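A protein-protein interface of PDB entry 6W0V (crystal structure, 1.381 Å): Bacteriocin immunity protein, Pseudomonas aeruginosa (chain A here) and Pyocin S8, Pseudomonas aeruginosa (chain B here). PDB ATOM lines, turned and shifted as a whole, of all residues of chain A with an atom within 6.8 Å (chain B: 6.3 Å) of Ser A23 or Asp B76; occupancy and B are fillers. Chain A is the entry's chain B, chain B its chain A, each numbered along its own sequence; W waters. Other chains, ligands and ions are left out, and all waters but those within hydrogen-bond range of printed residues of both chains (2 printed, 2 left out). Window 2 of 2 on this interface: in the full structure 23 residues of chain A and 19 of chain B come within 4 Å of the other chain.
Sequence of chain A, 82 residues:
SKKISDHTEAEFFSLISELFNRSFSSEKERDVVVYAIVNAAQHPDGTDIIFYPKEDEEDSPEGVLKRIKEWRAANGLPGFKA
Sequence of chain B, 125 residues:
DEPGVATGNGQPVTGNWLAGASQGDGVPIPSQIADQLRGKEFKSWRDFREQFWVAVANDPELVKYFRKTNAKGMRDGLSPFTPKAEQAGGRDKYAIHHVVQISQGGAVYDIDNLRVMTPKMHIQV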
ATOM      1  N   GLU A  18     -10.724 -25.498 -11.658  1.00  0.00           N
ATOM      2  CA  GLU A  18      -9.574 -24.640 -11.287  1.00  0.00           C
ATOM      3  C   GLU A  18      -8.286 -25.452 -11.404  1.00  0.00           C
ATOM      4  O   GLU A  18      -7.323 -24.938 -11.951  1.00  0.00           O
ATOM      5  CB  GLU A  18      -9.708 -24.107  -9.866  1.00  0.00           C
ATOM      6  CG  GLU A  18     -10.814 -23.090  -9.715  1.00  0.00           C
ATOM      7  CD  GLU A  18     -10.832 -22.397  -8.369  1.00  0.00           C
ATOM      8  OE1 GLU A  18      -9.758 -21.985  -7.916  1.00  0.00           O
ATOM      9  OE2 GLU A  18     -11.916 -22.273  -7.786  1.00  0.00           O
ATOM     10  N   LEU A  19      -8.277 -26.683 -10.905  1.00  0.00           N
ATOM     11  CA  LEU A  19      -7.040 -27.502 -10.891  1.00  0.00           C
ATOM     12  C   LEU A  19      -6.559 -27.766 -12.316  1.00  0.00           C
ATOM     13  O   LEU A  19      -5.351 -27.872 -12.510  1.00  0.00           O
ATOM     14  CB  LEU A  19      -7.282 -28.795 -10.122  1.00  0.00           C
ATOM     15  CG  LEU A  19      -7.670 -28.597  -8.663  1.00  0.00           C
ATOM     16  CD1 LEU A  19      -7.891 -29.930  -7.985  1.00  0.00           C
ATOM     17  CD2 LEU A  19      -6.608 -27.788  -7.926  1.00  0.00           C
ATOM     18  N   ASN A  21      -7.376 -25.745 -15.015  1.00  0.00           N
ATOM     19  CA  ASN A  21      -7.489 -24.544 -15.881  1.00  0.00           C
ATOM     20  C   ASN A  21      -6.868 -23.300 -15.241  1.00  0.00           C
ATOM     21  O   ASN A  21      -6.531 -22.387 -16.009  1.00  0.00           O
ATOM     22  CB  ASN A  21      -8.949 -24.316 -16.257  1.00  0.00           C
ATOM     23  CG  ASN A  21      -9.499 -25.510 -17.002  1.00  0.00           C
ATOM     24  OD1 ASN A  21      -8.865 -25.999 -17.933  1.00  0.00           O
ATOM     25  ND2 ASN A  21     -10.649 -26.008 -16.581  1.00  0.00           N
ATOM     26  N   ARG A  22      -6.759 -23.241 -13.912  1.00  0.00           N
ATOM     27  CA  ARG A  22      -6.327 -22.021 -13.180  1.00  0.00           C
ATOM     28  C   ARG A  22      -4.833 -22.148 -12.890  1.00  0.00           C
ATOM     29  O   ARG A  22      -4.365 -23.269 -12.628  1.00  0.00           O
ATOM     30  CB  ARG A  22      -7.126 -21.813 -11.888  1.00  0.00           C
ATOM     31  CG  ARG A  22      -6.434 -20.969 -10.825  1.00  0.00           C
ATOM     32  CD  ARG A  22      -7.330 -20.760  -9.616  1.00  0.00           C
ATOM     33  NE  ARG A  22      -6.809 -19.771  -8.680  1.00  0.00           N
ATOM     34  CZ  ARG A  22      -7.298 -19.526  -7.461  1.00  0.00           C
ATOM     35  NH1 ARG A  22      -8.325 -20.211  -6.983  1.00  0.00           N
ATOM     36  NH2 ARG A  22      -6.740 -18.590  -6.714  1.00  0.00           N
ATOM     37  N   SER A  23      -4.117 -21.031 -12.940  1.00  0.00           N
ATOM     38  CA  SER A  23      -2.732 -20.947 -12.430  1.00  0.00           C
ATOM     39  C   SER A  23      -2.774 -20.506 -10.968  1.00  0.00           C
ATOM     40  O   SER A  23      -3.280 -19.402 -10.669  1.00  0.00           O
ATOM     41  CB  SER A  23      -1.875 -20.058 -13.268  1.00  0.00           C
ATOM     42  OG  SER A  23      -1.493 -20.745 -14.444  1.00  0.00           O
ATOM     43  N   PHE A  24      -2.262 -21.353 -10.093  1.00  0.00           N
ATOM     44  CA  PHE A  24      -2.178 -21.060  -8.650  1.00  0.00           C
ATOM     45  C   PHE A  24      -0.857 -20.364  -8.385  1.00  0.00           C
ATOM     46  O   PHE A  24       0.162 -20.786  -8.945  1.00  0.00           O
ATOM     47  CB  PHE A  24      -2.341 -22.342  -7.853  1.00  0.00           C
ATOM     48  CG  PHE A  24      -3.743 -22.861  -7.951  1.00  0.00           C
ATOM     49  CD1 PHE A  24      -4.719 -22.346  -7.122  1.00  0.00           C
ATOM     50  CD2 PHE A  24      -4.084 -23.800  -8.904  1.00  0.00           C
ATOM     51  CE1 PHE A  24      -6.016 -22.812  -7.201  1.00  0.00           C
ATOM     52  CE2 PHE A  24      -5.386 -24.260  -8.985  1.00  0.00           C
ATOM     53  CZ  PHE A  24      -6.346 -23.755  -8.141  1.00  0.00           C
ATOM     54  N   SER A  25      -0.920 -19.322  -7.566  1.00  0.00           N
ATOM     55  CA  SER A  25       0.247 -18.486  -7.204  1.00  0.00           C
ATOM     56  C   SER A  25       1.157 -19.239  -6.240  1.00  0.00           C
ATOM     57  O   SER A  25       2.287 -18.809  -6.059  1.00  0.00           O
ATOM     58  CB  SER A  25      -0.186 -17.179  -6.623  1.00  0.00           C
ATOM     59  OG  SER A  25      -0.921 -17.380  -5.428  1.00  0.00           O
ATOM     60  N   SER A  26       0.675 -20.297  -5.608  1.00  0.00           N
ATOM     61  CA  SER A  26       1.476 -21.041  -4.614  1.00  0.00           C
ATOM     62  C   SER A  26       0.911 -22.435  -4.458  1.00  0.00           C
ATOM     63  O   SER A  26      -0.265 -22.666  -4.805  1.00  0.00           O
ATOM     64  CB  SER A  26       1.490 -20.337  -3.290  1.00  0.00           C
ATOM     65  OG  SER A  26       0.187 -20.382  -2.720  1.00  0.00           O
ATOM     66  N   GLU A  29      -2.104 -22.221  -2.122  1.00  0.00           N
ATOM     67  CA  GLU A  29      -3.361 -21.746  -2.732  1.00  0.00           C
ATOM     68  C   GLU A  29      -4.007 -22.928  -3.441  1.00  0.00           C
ATOM     69  O   GLU A  29      -5.227 -23.123  -3.311  1.00  0.00           O
ATOM     70  CB  GLU A  29      -3.098 -20.637  -3.730  1.00  0.00           C
ATOM     71  CG  GLU A  29      -4.364 -20.013  -4.227  1.00  0.00           C
ATOM     72  CD  GLU A  29      -4.037 -18.900  -5.185  1.00  0.00           C
ATOM     73  OE1 GLU A  29      -3.293 -19.160  -6.155  1.00  0.00           O
ATOM     74  OE2 GLU A  29      -4.487 -17.783  -4.924  1.00  0.00           O
ATOM     75  N   ARG A  30      -3.216 -23.694  -4.173  1.00  0.00           N
ATOM     76  CA  ARG A  30      -3.765 -24.851  -4.902  1.00  0.00           C
ATOM     77  C   ARG A  30      -4.264 -25.867  -3.891  1.00  0.00           C
ATOM     78  O   ARG A  30      -5.321 -26.454  -4.108  1.00  0.00           O
ATOM     79  CB  ARG A  30      -2.739 -25.502  -5.811  1.00  0.00           C
ATOM     80  CG  ARG A  30      -3.322 -26.701  -6.532  1.00  0.00           C
ATOM     81  CD  ARG A  30      -2.351 -27.396  -7.427  1.00  0.00           C
ATOM     82  NE  ARG A  30      -1.211 -27.844  -6.665  1.00  0.00           N
ATOM     83  CZ  ARG A  30      -0.225 -28.559  -7.149  1.00  0.00           C
ATOM     84  NH1 ARG A  30       0.782 -28.877  -6.356  1.00  0.00           N
ATOM     85  NH2 ARG A  30      -0.237 -28.947  -8.410  1.00  0.00           N
ATOM     86  N   ARG B  49      12.521 -24.677  -6.789  1.00  0.00           N
ATOM     87  CA  ARG B  49      11.513 -25.749  -6.859  1.00  0.00           C
ATOM     88  C   ARG B  49      10.572 -25.430  -8.018  1.00  0.00           C
ATOM     89  O   ARG B  49      10.209 -26.343  -8.770  1.00  0.00           O
ATOM     90  CB  ARG B  49      10.767 -25.865  -5.536  1.00  0.00           C
ATOM     91  CG  ARG B  49       9.663 -26.904  -5.592  1.00  0.00           C
ATOM     92  CD  ARG B  49       8.349 -26.247  -5.896  1.00  0.00           C
ATOM     93  NE  ARG B  49       7.933 -25.480  -4.740  1.00  0.00           N
ATOM     94  CZ  ARG B  49       6.951 -24.598  -4.764  1.00  0.00           C
ATOM     95  NH1 ARG B  49       6.615 -23.942  -3.671  1.00  0.00           N
ATOM     96  NH2 ARG B  49       6.296 -24.389  -5.893  1.00  0.00           N
ATOM     97  N   GLU B  50      10.154 -24.179  -8.126  1.00  0.00           N
ATOM     98  CA  GLU B  50       9.219 -23.795  -9.204  1.00  0.00           C
ATOM     99  C   GLU B  50       9.887 -24.025 -10.552  1.00  0.00           C
ATOM    100  O   GLU B  50       9.305 -24.628 -11.431  1.00  0.00           O
ATOM    101  CB  GLU B  50       8.815 -22.344  -9.077  1.00  0.00           C
ATOM    102  CG  GLU B  50       7.860 -22.131  -7.949  1.00  0.00           C
ATOM    103  CD  GLU B  50       7.364 -20.709  -7.868  1.00  0.00           C
ATOM    104  OE1 GLU B  50       7.770 -19.894  -8.722  1.00  0.00           O
ATOM    105  OE2 GLU B  50       6.578 -20.428  -6.958  1.00  0.00           O
ATOM    106  N   VAL B  54       8.644 -26.494 -13.376  1.00  0.00           N
ATOM    107  CA  VAL B  54       8.352 -25.880 -14.694  1.00  0.00           C
ATOM    108  C   VAL B  54       9.177 -26.604 -15.746  1.00  0.00           C
ATOM    109  O   VAL B  54       8.657 -26.918 -16.803  1.00  0.00           O
ATOM    110  CB  VAL B  54       8.621 -24.373 -14.692  1.00  0.00           C
ATOM    111  CG1 VAL B  54       8.691 -23.801 -16.093  1.00  0.00           C
ATOM    112  CG2 VAL B  54       7.581 -23.653 -13.861  1.00  0.00           C
ATOM    113  N   ALA B  57       7.697 -29.965 -16.387  1.00  0.00           N
ATOM    114  CA  ALA B  57       6.451 -29.819 -17.176  1.00  0.00           C
ATOM    115  C   ALA B  57       6.816 -29.481 -18.619  1.00  0.00           C
ATOM    116  O   ALA B  57       6.063 -29.821 -19.511  1.00  0.00           O
ATOM    117  CB  ALA B  57       5.568 -28.763 -16.589  1.00  0.00           C
ATOM    118  N   ALA B  71       0.475 -31.837 -14.248  1.00  0.00           N
ATOM    119  CA  ALA B  71       1.239 -31.135 -15.295  1.00  0.00           C
ATOM    120  C   ALA B  71       0.899 -29.647 -15.233  1.00  0.00           C
ATOM    121  O   ALA B  71       1.794 -28.822 -15.339  1.00  0.00           O
ATOM    122  CB  ALA B  71       0.946 -31.703 -16.648  1.00  0.00           C
ATOM    123  N   LYS B  72      -0.375 -29.319 -15.077  1.00  0.00           N
ATOM    124  CA  LYS B  72      -0.829 -27.920 -15.008  1.00  0.00           C
ATOM    125  C   LYS B  72      -0.130 -27.246 -13.837  1.00  0.00           C
ATOM    126  O   LYS B  72       0.420 -26.159 -14.016  1.00  0.00           O
ATOM    127  CB  LYS B  72      -2.336 -27.838 -14.789  1.00  0.00           C
ATOM    128  CG  LYS B  72      -2.857 -26.418 -14.656  1.00  0.00           C
ATOM    129  CD  LYS B  72      -2.769 -25.645 -15.934  1.00  0.00           C
ATOM    130  CE  LYS B  72      -3.263 -24.223 -15.788  1.00  0.00           C
ATOM    131  NZ  LYS B  72      -3.200 -23.492 -17.075  1.00  0.00           N
ATOM    132  N   GLY B  73      -0.156 -27.895 -12.683  1.00  0.00           N
ATOM    133  CA  GLY B  73       0.491 -27.339 -11.484  1.00  0.00           C
ATOM    134  C   GLY B  73       1.961 -27.151 -11.743  1.00  0.00           C
ATOM    135  O   GLY B  73       2.498 -26.101 -11.374  1.00  0.00           O
ATOM    136  N   MET B  74       2.586 -28.140 -12.363  1.00  0.00           N
ATOM    137  CA  MET B  74       4.040 -28.076 -12.624  1.00  0.00           C
ATOM    138  C   MET B  74       4.347 -26.909 -13.551  1.00  0.00           C
ATOM    139  O   MET B  74       5.358 -26.270 -13.359  1.00  0.00           O
ATOM    140  CB  MET B  74       4.539 -29.380 -13.224  1.00  0.00           C
ATOM    141  CG  MET B  74       4.590 -30.462 -12.206  1.00  0.00           C
ATOM    142  SD  MET B  74       5.711 -31.812 -12.661  1.00  0.00           S
ATOM    143  CE  MET B  74       5.576 -31.824 -14.449  1.00  0.00           C
ATOM    144  N   ARG B  75       3.489 -26.592 -14.504  1.00  0.00           N
ATOM    145  CA  ARG B  75       3.725 -25.438 -15.398  1.00  0.00           C
ATOM    146  C   ARG B  75       3.682 -24.146 -14.581  1.00  0.00           C
ATOM    147  O   ARG B  75       4.276 -23.158 -15.026  1.00  0.00           O
ATOM    148  CB  ARG B  75       2.716 -25.431 -16.539  1.00  0.00           C
ATOM    149  CG  ARG B  75       3.015 -26.505 -17.567  1.00  0.00           C
ATOM    150  CD  ARG B  75       2.188 -26.316 -18.817  1.00  0.00           C
ATOM    151  NE  ARG B  75       0.756 -26.481 -18.596  1.00  0.00           N
ATOM    152  CZ  ARG B  75       0.123 -27.648 -18.554  1.00  0.00           C
ATOM    153  NH1 ARG B  75      -1.187 -27.670 -18.380  1.00  0.00           N
ATOM    154  NH2 ARG B  75       0.783 -28.785 -18.688  1.00  0.00           N
ATOM    155  N   ASP B  76       3.032 -24.179 -13.421  1.00  0.00           N
ATOM    156  CA  ASP B  76       2.964 -23.043 -12.469  1.00  0.00           C
ATOM    157  C   ASP B  76       4.094 -23.162 -11.455  1.00  0.00           C
ATOM    158  O   ASP B  76       4.140 -22.321 -10.550  1.00  0.00           O
ATOM    159  CB  ASP B  76       1.643 -23.021 -11.705  1.00  0.00           C
ATOM    160  CG  ASP B  76       0.444 -22.682 -12.554  1.00  0.00           C
ATOM    161  OD1 ASP B  76       0.642 -22.084 -13.627  1.00  0.00           O
ATOM    162  OD2 ASP B  76      -0.670 -23.040 -12.129  1.00  0.00           O
ATOM    163  N   GLY B  77       4.931 -24.184 -11.593  1.00  0.00           N
ATOM    164  CA  GLY B  77       6.063 -24.424 -10.684  1.00  0.00           C
ATOM    165  C   GLY B  77       5.624 -25.134  -9.427  1.00  0.00           C
ATOM    166  O   GLY B  77       6.386 -25.179  -8.477  1.00  0.00           O
ATOM    167  N   LEU B  78       4.419 -25.701  -9.410  1.00  0.00           N
ATOM    168  CA  LEU B  78       3.887 -26.372  -8.211  1.00  0.00           C
ATOM    169  C   LEU B  78       4.281 -27.838  -8.236  1.00  0.00           C
ATOM    170  O   LEU B  78       4.200 -28.482  -9.291  1.00  0.00           O
ATOM    171  CB  LEU B  78       2.370 -26.248  -8.182  1.00  0.00           C
ATOM    172  CG  LEU B  78       1.855 -24.829  -8.338  1.00  0.00           C
ATOM    173  CD1 LEU B  78       0.341 -24.833  -8.360  1.00  0.00           C
ATOM    174  CD2 LEU B  78       2.377 -23.933  -7.230  1.00  0.00           C
HETATM  175  O   HOH W   1       1.849 -29.975  -9.861  1.00  0.00           O
HETATM  176  O   HOH W   2      -3.532 -20.806 -16.249  1.00  0.00           O
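Water W2 lies within hydrogen-bond range of the side-chain hydroxyl (OG) of Ser A23, the side-chain amino group (NZ) of Lys B72 and the backbone carbonyl oxygen (O) of Asn A21. Water W1 lies within hydrogen-bond range of the guanidinium group of Arg A30, the backbone carbonyl oxygen of Leu B78 and the backbone NH of Met B74.
O of Gly B73 sits at hydrogen-bond distance from N of Leu B78 (2.8 Å). The side-chain carboxylate (OE1) of Glu A18 lies within salt-bridge range of the guanidinium group (NH1) of Arg A22 (2.5 Å). The guanidinium group (NH2) of Arg A22 is in salt-bridge range of the side-chain carboxylate (OE2) of Glu A29 (3.0 Å). N of Glu A29 is in hydrogen-bond range of OG of Ser A26 (3.0 Å).
Ser A23 touches just one residue of chain B: Asp B76. Asp B76 touches just these residues of chain A: Arg A22 (3.7 Å), Ser A23 (2.6 Å) and Phe A24 (3.1 Å). Printed residues of chain B within 4 Å of Leu A19: Lys B72 (3.6 Å). Printed residues of chain B within 4 Å of Arg A22: Lys B72 (3.5 Å) and Asp B76 (3.7 Å). Of the printed residues of chain B, Asn A21 touches Lys B72.
Among the printed residues, merely in contact across the chains: Ser A26 with Leu B78 (3.5 Å), Arg A22 with Lys B72 (3.5 Å), Arg A30 with Gly B73 (3.5 Å), Arg A30 with Leu B78 (3.6 Å), Leu A19 with Lys B72 (3.6 Å), Asn A21 with Lys B72 (3.7 Å), Phe A24 with Leu B78 (3.7 Å) and Arg A22 with Asp B76 (3.7 Å).
The side-chain hydroxyl (OG) of Ser A23 is in hydrogen-bond range of the side-chain carboxylate (OD1) of Asp B76 (2.6 Å). OD2 of Asp B76 sits at hydrogen-bond distance from N of Phe A24, 3.1 Å away.
Of the 12 printed residues of chain B, 4 touch a printed residue of chain A. Printed residues of chain B that touch a printed residue of chain A: Lys B72, Gly B73, Asp B76 and Leu B78. Hydrophobic or aromatic side chains of chain B that line the printed part of chain A: Leu B78. Of the 10 printed residues of chain A, 7 touch a printed residue of chain B. Hydrophobic or aromatic side chains of chain A that line the printed part of chain B: Phe A24.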
